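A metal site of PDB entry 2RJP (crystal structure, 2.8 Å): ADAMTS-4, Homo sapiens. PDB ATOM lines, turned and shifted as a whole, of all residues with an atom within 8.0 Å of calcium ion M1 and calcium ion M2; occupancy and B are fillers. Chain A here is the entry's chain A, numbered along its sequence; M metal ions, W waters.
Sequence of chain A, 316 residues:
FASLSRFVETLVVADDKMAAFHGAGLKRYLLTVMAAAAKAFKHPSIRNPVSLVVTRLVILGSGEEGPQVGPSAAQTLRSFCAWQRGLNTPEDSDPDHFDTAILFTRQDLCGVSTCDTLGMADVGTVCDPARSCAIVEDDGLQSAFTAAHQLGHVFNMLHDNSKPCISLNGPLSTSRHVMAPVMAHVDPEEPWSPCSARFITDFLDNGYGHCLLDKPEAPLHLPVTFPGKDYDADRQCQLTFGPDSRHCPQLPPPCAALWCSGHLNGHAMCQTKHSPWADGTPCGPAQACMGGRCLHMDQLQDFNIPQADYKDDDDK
The backbone NH of Thr 100 sits at hydrogen-bond distance from the backbone carbonyl oxygen of Glu 9 (3.2 Å).
The side-chain sulfur of Cys 211 forms a disulfide with the side-chain sulfur of Cys 127 (2.0 Å).
Within 4 Å of calcium ion M1: Glu 9, Asp 92, Asp 99, Cys 211 and Asp 214.
The nearest printed residue that does not touch calcium ion M1 is Leu 212 (4.2 Å).
Within 4 Å of calcium ion M2: Glu 9, Asp 92 and Asp 214.
The nearest printed residue that does not touch calcium ion M2 is Asp 94 (4.3 Å).
Calcium ion M1 is bound by OE1 of Glu 9 (2.4 Å), OD2 of Asp 92 (2.4 Å), O of Cys 211 (2.4 Å), OD1 of Asp 214 (2.4 Å) and OD2 of Asp 99 (2.5 Å).
Calcium ion M1 has five donor atoms within binding distance.
Slightly farther from calcium ion M1 lies OD1 of Asp 99 (3.0 Å).
Water W1 is bound to calcium ion M2.
OD1 of Asp 92 binds calcium ion M2 (2.5 Å).
OD2 of Asp 214 is bound to calcium ion M2 (2.7 Å).
O of Asp 92 is bound to calcium ion M2.
OE1 of Glu 9 is bound to calcium ion M2, 2.8 Å away.
Calcium ion M2 is bound by OE2 of Glu 9.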
ATOM      1  N   ARG A   6     -10.247  -3.146 -16.041  1.00  0.00           N
ATOM      2  CA  ARG A   6     -11.373  -2.234 -16.113  1.00  0.00           C
ATOM      3  C   ARG A   6     -12.671  -2.919 -15.729  1.00  0.00           C
ATOM      4  O   ARG A   6     -12.869  -4.098 -16.022  1.00  0.00           O
ATOM      5  CB  ARG A   6     -11.456  -1.617 -17.510  1.00  0.00           C
ATOM      6  CG  ARG A   6     -10.462  -0.452 -17.684  1.00  0.00           C
ATOM      7  CD  ARG A   6      -9.955  -0.288 -19.113  1.00  0.00           C
ATOM      8  NE  ARG A   6      -8.697   0.459 -19.155  1.00  0.00           N
ATOM      9  CZ  ARG A   6      -8.606   1.792 -19.110  1.00  0.00           C
ATOM     10  NH1 ARG A   6      -9.685   2.549 -19.031  1.00  0.00           N
ATOM     11  NH2 ARG A   6      -7.415   2.372 -19.143  1.00  0.00           N
ATOM     12  N   PHE A   7     -13.544  -2.172 -15.059  1.00  0.00           N
ATOM     13  CA  PHE A   7     -14.818  -2.697 -14.585  1.00  0.00           C
ATOM     14  C   PHE A   7     -15.961  -1.835 -15.099  1.00  0.00           C
ATOM     15  O   PHE A   7     -15.969  -0.622 -14.903  1.00  0.00           O
ATOM     16  CB  PHE A   7     -14.822  -2.762 -13.050  1.00  0.00           C
ATOM     17  CG  PHE A   7     -13.679  -3.553 -12.497  1.00  0.00           C
ATOM     18  CD1 PHE A   7     -12.467  -2.930 -12.178  1.00  0.00           C
ATOM     19  CD2 PHE A   7     -13.791  -4.922 -12.304  1.00  0.00           C
ATOM     20  CE1 PHE A   7     -11.392  -3.656 -11.672  1.00  0.00           C
ATOM     21  CE2 PHE A   7     -12.719  -5.664 -11.806  1.00  0.00           C
ATOM     22  CZ  PHE A   7     -11.512  -5.032 -11.489  1.00  0.00           C
ATOM     23  N   VAL A   8     -16.913  -2.471 -15.776  1.00  0.00           N
ATOM     24  CA  VAL A   8     -18.093  -1.767 -16.279  1.00  0.00           C
ATOM     25  C   VAL A   8     -19.259  -2.002 -15.342  1.00  0.00           C
ATOM     26  O   VAL A   8     -19.914  -3.045 -15.387  1.00  0.00           O
ATOM     27  CB  VAL A   8     -18.494  -2.171 -17.720  1.00  0.00           C
ATOM     28  CG1 VAL A   8     -19.699  -1.342 -18.194  1.00  0.00           C
ATOM     29  CG2 VAL A   8     -17.337  -2.009 -18.678  1.00  0.00           C
ATOM     30  N   GLU A   9     -19.497  -1.030 -14.470  1.00  0.00           N
ATOM     31  CA  GLU A   9     -20.554  -1.141 -13.480  1.00  0.00           C
ATOM     32  C   GLU A   9     -21.867  -0.864 -14.204  1.00  0.00           C
ATOM     33  O   GLU A   9     -22.069   0.235 -14.742  1.00  0.00           O
ATOM     34  CB  GLU A   9     -20.290  -0.189 -12.311  1.00  0.00           C
ATOM     35  CG  GLU A   9     -18.989  -0.519 -11.560  1.00  0.00           C
ATOM     36  CD  GLU A   9     -18.606   0.524 -10.515  1.00  0.00           C
ATOM     37  OE1 GLU A   9     -18.142   1.626 -10.885  1.00  0.00           O
ATOM     38  OE2 GLU A   9     -18.720   0.226  -9.300  1.00  0.00           O
ATOM     39  N   THR A  10     -22.736  -1.878 -14.234  1.00  0.00           N
ATOM     40  CA  THR A  10     -23.884  -1.895 -15.129  1.00  0.00           C
ATOM     41  C   THR A  10     -25.209  -1.884 -14.420  1.00  0.00           C
ATOM     42  O   THR A  10     -25.401  -2.582 -13.424  1.00  0.00           O
ATOM     43  CB  THR A  10     -23.831  -3.129 -16.050  1.00  0.00           C
ATOM     44  OG1 THR A  10     -22.573  -3.147 -16.745  1.00  0.00           O
ATOM     45  CG2 THR A  10     -24.979  -3.111 -17.063  1.00  0.00           C
ATOM     46  N   THR A  55     -24.161  -4.147 -11.113  1.00  0.00           N
ATOM     47  CA  THR A  55     -24.213  -3.563  -9.786  1.00  0.00           C
ATOM     48  C   THR A  55     -25.642  -3.229  -9.360  1.00  0.00           C
ATOM     49  O   THR A  55     -25.964  -3.206  -8.165  1.00  0.00           O
ATOM     50  CB  THR A  55     -23.278  -2.327  -9.631  1.00  0.00           C
ATOM     51  OG1 THR A  55     -23.714  -1.279 -10.500  1.00  0.00           O
ATOM     52  CG2 THR A  55     -21.845  -2.685  -9.961  1.00  0.00           C
ATOM     53  N   THR A  89     -25.906   8.827  -9.939  1.00  0.00           N
ATOM     54  CA  THR A  89     -25.444   9.666  -8.834  1.00  0.00           C
ATOM     55  C   THR A  89     -24.259  10.515  -9.296  1.00  0.00           C
ATOM     56  O   THR A  89     -23.505  10.097 -10.172  1.00  0.00           O
ATOM     57  CB  THR A  89     -24.971   8.833  -7.619  1.00  0.00           C
ATOM     58  OG1 THR A  89     -23.707   8.229  -7.917  1.00  0.00           O
ATOM     59  CG2 THR A  89     -25.990   7.743  -7.256  1.00  0.00           C
ATOM     60  N   GLU A  91     -21.105  11.254  -8.109  1.00  0.00           N
ATOM     61  CA  GLU A  91     -19.761  10.660  -8.116  1.00  0.00           C
ATOM     62  C   GLU A  91     -19.731   9.133  -8.240  1.00  0.00           C
ATOM     63  O   GLU A  91     -20.715   8.450  -7.927  1.00  0.00           O
ATOM     64  CB  GLU A  91     -18.957  11.111  -6.875  1.00  0.00           C
ATOM     65  CG  GLU A  91     -18.227  12.447  -7.072  1.00  0.00           C
ATOM     66  CD  GLU A  91     -17.839  13.132  -5.767  1.00  0.00           C
ATOM     67  OE1 GLU A  91     -18.382  12.751  -4.704  1.00  0.00           O
ATOM     68  OE2 GLU A  91     -17.012  14.064  -5.810  1.00  0.00           O
ATOM     69  N   ASP A  92     -18.593   8.604  -8.695  1.00  0.00           N
ATOM     70  CA  ASP A  92     -18.400   7.157  -8.856  1.00  0.00           C
ATOM     71  C   ASP A  92     -17.865   6.517  -7.573  1.00  0.00           C
ATOM     72  O   ASP A  92     -17.624   5.304  -7.502  1.00  0.00           O
ATOM     73  CB  ASP A  92     -17.461   6.856 -10.047  1.00  0.00           C
ATOM     74  CG  ASP A  92     -17.669   5.459 -10.623  1.00  0.00           C
ATOM     75  OD1 ASP A  92     -18.503   4.683 -10.087  1.00  0.00           O
ATOM     76  OD2 ASP A  92     -17.008   5.121 -11.623  1.00  0.00           O
ATOM     77  N   SER A  93     -17.685   7.343  -6.545  1.00  0.00           N
ATOM     78  CA  SER A  93     -17.360   6.868  -5.208  1.00  0.00           C
ATOM     79  C   SER A  93     -18.578   6.139  -4.606  1.00  0.00           C
ATOM     80  O   SER A  93     -18.423   5.145  -3.896  1.00  0.00           O
ATOM     81  CB  SER A  93     -16.933   8.039  -4.331  1.00  0.00           C
ATOM     82  OG  SER A  93     -17.006   7.718  -2.956  1.00  0.00           O
ATOM     83  N   ASP A  94     -19.764   6.660  -4.908  1.00  0.00           N
ATOM     84  CA  ASP A  94     -21.010   6.165  -4.334  1.00  0.00           C
ATOM     85  C   ASP A  94     -21.385   4.800  -4.911  1.00  0.00           C
ATOM     86  O   ASP A  94     -21.558   4.666  -6.128  1.00  0.00           O
ATOM     87  CB  ASP A  94     -22.134   7.179  -4.564  1.00  0.00           C
ATOM     88  CG  ASP A  94     -23.330   6.952  -3.662  1.00  0.00           C
ATOM     89  OD1 ASP A  94     -24.018   5.920  -3.834  1.00  0.00           O
ATOM     90  OD2 ASP A  94     -23.591   7.798  -2.783  1.00  0.00           O
ATOM     91  N   PRO A  95     -21.517   3.766  -4.051  1.00  0.00           N
ATOM     92  CA  PRO A  95     -21.836   2.390  -4.467  1.00  0.00           C
ATOM     93  C   PRO A  95     -23.095   2.252  -5.335  1.00  0.00           C
ATOM     94  O   PRO A  95     -23.363   1.172  -5.854  1.00  0.00           O
ATOM     95  CB  PRO A  95     -22.048   1.654  -3.133  1.00  0.00           C
ATOM     96  CG  PRO A  95     -22.213   2.735  -2.108  1.00  0.00           C
ATOM     97  CD  PRO A  95     -21.382   3.868  -2.588  1.00  0.00           C
ATOM     98  N   ASP A  96     -23.847   3.344  -5.479  1.00  0.00           N
ATOM     99  CA  ASP A  96     -25.040   3.357  -6.322  1.00  0.00           C
ATOM    100  C   ASP A  96     -24.800   3.910  -7.727  1.00  0.00           C
ATOM    101  O   ASP A  96     -25.708   3.861  -8.563  1.00  0.00           O
ATOM    102  CB  ASP A  96     -26.175   4.114  -5.629  1.00  0.00           C
ATOM    103  CG  ASP A  96     -27.045   3.217  -4.752  1.00  0.00           C
ATOM    104  OD1 ASP A  96     -27.241   2.034  -5.125  1.00  0.00           O
ATOM    105  OD2 ASP A  96     -27.543   3.688  -3.716  1.00  0.00           O
ATOM    106  N   HIS A  97     -23.592   4.410  -8.000  1.00  0.00           N
ATOM    107  CA  HIS A  97     -23.214   4.904  -9.321  1.00  0.00           C
ATOM    108  C   HIS A  97     -23.015   3.758 -10.302  1.00  0.00           C
ATOM    109  O   HIS A  97     -22.496   2.707  -9.923  1.00  0.00           O
ATOM    110  CB  HIS A  97     -21.933   5.742  -9.253  1.00  0.00           C
ATOM    111  CG  HIS A  97     -21.589   6.446 -10.528  1.00  0.00           C
ATOM    112  ND1 HIS A  97     -22.046   7.705 -10.832  1.00  0.00           N
ATOM    113  CD2 HIS A  97     -20.829   6.053 -11.581  1.00  0.00           C
ATOM    114  CE1 HIS A  97     -21.586   8.066 -12.012  1.00  0.00           C
ATOM    115  NE2 HIS A  97     -20.843   7.087 -12.486  1.00  0.00           N
ATOM    116  N   PHE A  98     -23.438   3.953 -11.544  1.00  0.00           N
ATOM    117  CA  PHE A  98     -23.235   2.975 -12.612  1.00  0.00           C
ATOM    118  C   PHE A  98     -22.636   3.627 -13.854  1.00  0.00           C
ATOM    119  O   PHE A  98     -22.924   4.782 -14.155  1.00  0.00           O
ATOM    120  CB  PHE A  98     -24.526   2.238 -12.972  1.00  0.00           C
ATOM    121  CG  PHE A  98     -25.689   3.146 -13.332  1.00  0.00           C
ATOM    122  CD1 PHE A  98     -25.855   3.604 -14.630  1.00  0.00           C
ATOM    123  CD2 PHE A  98     -26.613   3.530 -12.365  1.00  0.00           C
ATOM    124  CE1 PHE A  98     -26.918   4.438 -14.968  1.00  0.00           C
ATOM    125  CE2 PHE A  98     -27.685   4.361 -12.684  1.00  0.00           C
ATOM    126  CZ  PHE A  98     -27.837   4.815 -13.990  1.00  0.00           C
ATOM    127  N   ASP A  99     -21.809   2.875 -14.569  1.00  0.00           N
ATOM    128  CA  ASP A  99     -21.094   3.429 -15.723  1.00  0.00           C
ATOM    129  C   ASP A  99     -21.810   3.202 -17.061  1.00  0.00           C
ATOM    130  O   ASP A  99     -21.431   3.804 -18.073  1.00  0.00           O
ATOM    131  CB  ASP A  99     -19.673   2.863 -15.788  1.00  0.00           C
ATOM    132  CG  ASP A  99     -18.886   3.126 -14.509  1.00  0.00           C
ATOM    133  OD1 ASP A  99     -18.667   4.313 -14.134  1.00  0.00           O
ATOM    134  OD2 ASP A  99     -18.460   2.127 -13.883  1.00  0.00           O
ATOM    135  N   THR A 100     -22.821   2.343 -17.069  1.00  0.00           N
ATOM    136  CA  THR A 100     -23.521   1.989 -18.304  1.00  0.00           C
ATOM    137  C   THR A 100     -24.924   1.490 -17.980  1.00  0.00           C
ATOM    138  O   THR A 100     -25.140   0.899 -16.923  1.00  0.00           O
ATOM    139  CB  THR A 100     -22.721   0.923 -19.125  1.00  0.00           C
ATOM    140  OG1 THR A 100     -22.613   1.332 -20.490  1.00  0.00           O
ATOM    141  CG2 THR A 100     -23.351  -0.472 -19.052  1.00  0.00           C
ATOM    142  N   CYS A 127     -18.127   6.560 -20.676  1.00  0.00           N
ATOM    143  CA  CYS A 127     -17.899   7.389 -19.501  1.00  0.00           C
ATOM    144  C   CYS A 127     -18.688   8.711 -19.502  1.00  0.00           C
ATOM    145  O   CYS A 127     -18.412   9.625 -18.702  1.00  0.00           O
ATOM    146  CB  CYS A 127     -16.408   7.624 -19.297  1.00  0.00           C
ATOM    147  SG  CYS A 127     -15.546   6.148 -18.726  1.00  0.00           S
ATOM    148  N   GLY A 209     -12.073   5.820 -21.053  1.00  0.00           N
ATOM    149  CA  GLY A 209     -12.564   4.816 -20.111  1.00  0.00           C
ATOM    150  C   GLY A 209     -12.215   5.101 -18.656  1.00  0.00           C
ATOM    151  O   GLY A 209     -12.184   4.182 -17.838  1.00  0.00           O
ATOM    152  N   HIS A 210     -11.968   6.368 -18.341  1.00  0.00           N
ATOM    153  CA  HIS A 210     -11.533   6.773 -16.998  1.00  0.00           C
ATOM    154  C   HIS A 210     -12.480   6.293 -15.899  1.00  0.00           C
ATOM    155  O   HIS A 210     -12.034   5.920 -14.810  1.00  0.00           O
ATOM    156  CB  HIS A 210     -11.341   8.294 -16.922  1.00  0.00           C
ATOM    157  CG  HIS A 210     -12.597   9.077 -17.170  1.00  0.00           C
ATOM    158  ND1 HIS A 210     -13.444   9.699 -16.314  1.00  0.00           N
ATOM    159  CD2 HIS A 210     -13.099   9.298 -18.434  1.00  0.00           C
ATOM    160  CE1 HIS A 210     -14.432  10.279 -17.073  1.00  0.00           C
ATOM    161  NE2 HIS A 210     -14.206  10.025 -18.344  1.00  0.00           N
ATOM    162  N   CYS A 211     -13.772   6.297 -16.202  1.00  0.00           N
ATOM    163  CA  CYS A 211     -14.808   5.907 -15.258  1.00  0.00           C
ATOM    164  C   CYS A 211     -14.852   4.404 -14.936  1.00  0.00           C
ATOM    165  O   CYS A 211     -15.719   3.961 -14.191  1.00  0.00           O
ATOM    166  CB  CYS A 211     -16.184   6.349 -15.770  1.00  0.00           C
ATOM    167  SG  CYS A 211     -16.738   5.426 -17.237  1.00  0.00           S
ATOM    168  N   LEU A 212     -13.921   3.645 -15.507  1.00  0.00           N
ATOM    169  CA  LEU A 212     -13.972   2.186 -15.406  1.00  0.00           C
ATOM    170  C   LEU A 212     -12.867   1.613 -14.535  1.00  0.00           C
ATOM    171  O   LEU A 212     -12.716   0.389 -14.451  1.00  0.00           O
ATOM    172  CB  LEU A 212     -13.902   1.540 -16.793  1.00  0.00           C
ATOM    173  CG  LEU A 212     -14.906   1.910 -17.887  1.00  0.00           C
ATOM    174  CD1 LEU A 212     -14.477   1.273 -19.179  1.00  0.00           C
ATOM    175  CD2 LEU A 212     -16.337   1.489 -17.517  1.00  0.00           C
ATOM    176  N   LEU A 213     -12.117   2.488 -13.885  1.00  0.00           N
ATOM    177  CA  LEU A 213     -10.913   2.070 -13.170  1.00  0.00           C
ATOM    178  C   LEU A 213     -11.150   1.547 -11.749  1.00  0.00           C
ATOM    179  O   LEU A 213     -10.389   0.711 -11.268  1.00  0.00           O
ATOM    180  CB  LEU A 213      -9.863   3.190 -13.169  1.00  0.00           C
ATOM    181  CG  LEU A 213      -9.205   3.488 -14.523  1.00  0.00           C
ATOM    182  CD1 LEU A 213      -8.521   4.841 -14.503  1.00  0.00           C
ATOM    183  CD2 LEU A 213      -8.218   2.385 -14.923  1.00  0.00           C
ATOM    184  N   ASP A 214     -12.206   2.031 -11.086  1.00  0.00           N
ATOM    185  CA  ASP A 214     -12.560   1.572  -9.738  1.00  0.00           C
ATOM    186  C   ASP A 214     -13.232   0.185  -9.721  1.00  0.00           C
ATOM    187  O   ASP A 214     -13.935  -0.180 -10.670  1.00  0.00           O
ATOM    188  CB  ASP A 214     -13.475   2.592  -9.043  1.00  0.00           C
ATOM    189  CG  ASP A 214     -14.824   2.728  -9.738  1.00  0.00           C
ATOM    190  OD1 ASP A 214     -14.855   3.254 -10.871  1.00  0.00           O
ATOM    191  OD2 ASP A 214     -15.843   2.291  -9.162  1.00  0.00           O
ATOM    192  N   LYS A 215     -13.021  -0.550  -8.639  1.00  0.00           N
ATOM    193  CA  LYS A 215     -13.628  -1.872  -8.483  1.00  0.00           C
ATOM    194  C   LYS A 215     -14.987  -1.760  -7.772  1.00  0.00           C
ATOM    195  O   LYS A 215     -15.118  -1.046  -6.777  1.00  0.00           O
ATOM    196  CB  LYS A 215     -12.690  -2.821  -7.722  1.00  0.00           C
ATOM    197  CG  LYS A 215     -12.979  -4.291  -7.989  1.00  0.00           C
ATOM    198  CD  LYS A 215     -12.156  -5.249  -7.136  1.00  0.00           C
ATOM    199  CE  LYS A 215     -12.580  -6.698  -7.389  1.00  0.00           C
ATOM    200  NZ  LYS A 215     -12.029  -7.629  -6.355  1.00  0.00           N
ATOM    201  N   PRO A 216     -16.015  -2.476  -8.291  1.00  0.00           N
ATOM    202  CA  PRO A 216     -17.381  -2.338  -7.778  1.00  0.00           C
ATOM    203  C   PRO A 216     -17.546  -2.753  -6.316  1.00  0.00           C
ATOM    204  O   PRO A 216     -16.928  -3.733  -5.867  1.00  0.00           O
ATOM    205  CB  PRO A 216     -18.191  -3.252  -8.693  1.00  0.00           C
ATOM    206  CG  PRO A 216     -17.207  -4.264  -9.179  1.00  0.00           C
ATOM    207  CD  PRO A 216     -15.944  -3.473  -9.369  1.00  0.00           C
ATOM    208  N   GLU A 217     -18.392  -2.026  -5.599  1.00  0.00           N
ATOM    209  CA  GLU A 217     -18.664  -2.251  -4.177  1.00  0.00           C
ATOM    210  C   GLU A 217     -19.134  -3.682  -3.879  1.00  0.00           C
ATOM    211  O   GLU A 217     -18.475  -4.420  -3.138  1.00  0.00           O
ATOM    212  CB  GLU A 217     -19.686  -1.237  -3.675  1.00  0.00           C
ATOM    213  CG  GLU A 217     -20.134  -1.417  -2.227  1.00  0.00           C
ATOM    214  CD  GLU A 217     -19.284  -0.647  -1.246  1.00  0.00           C
ATOM    215  OE1 GLU A 217     -18.030  -0.706  -1.345  1.00  0.00           O
ATOM    216  OE2 GLU A 217     -19.869   0.036  -0.373  1.00  0.00           O
HETATM  217 CA    CA M   1     -16.722   2.864 -12.319  1.00  0.00          CA
HETATM  218 CA    CA M   2     -18.341   2.842  -8.389  1.00  0.00          CA
HETATM  219  O   HOH W   1     -17.201   1.201  -7.042  1.00  0.00           O
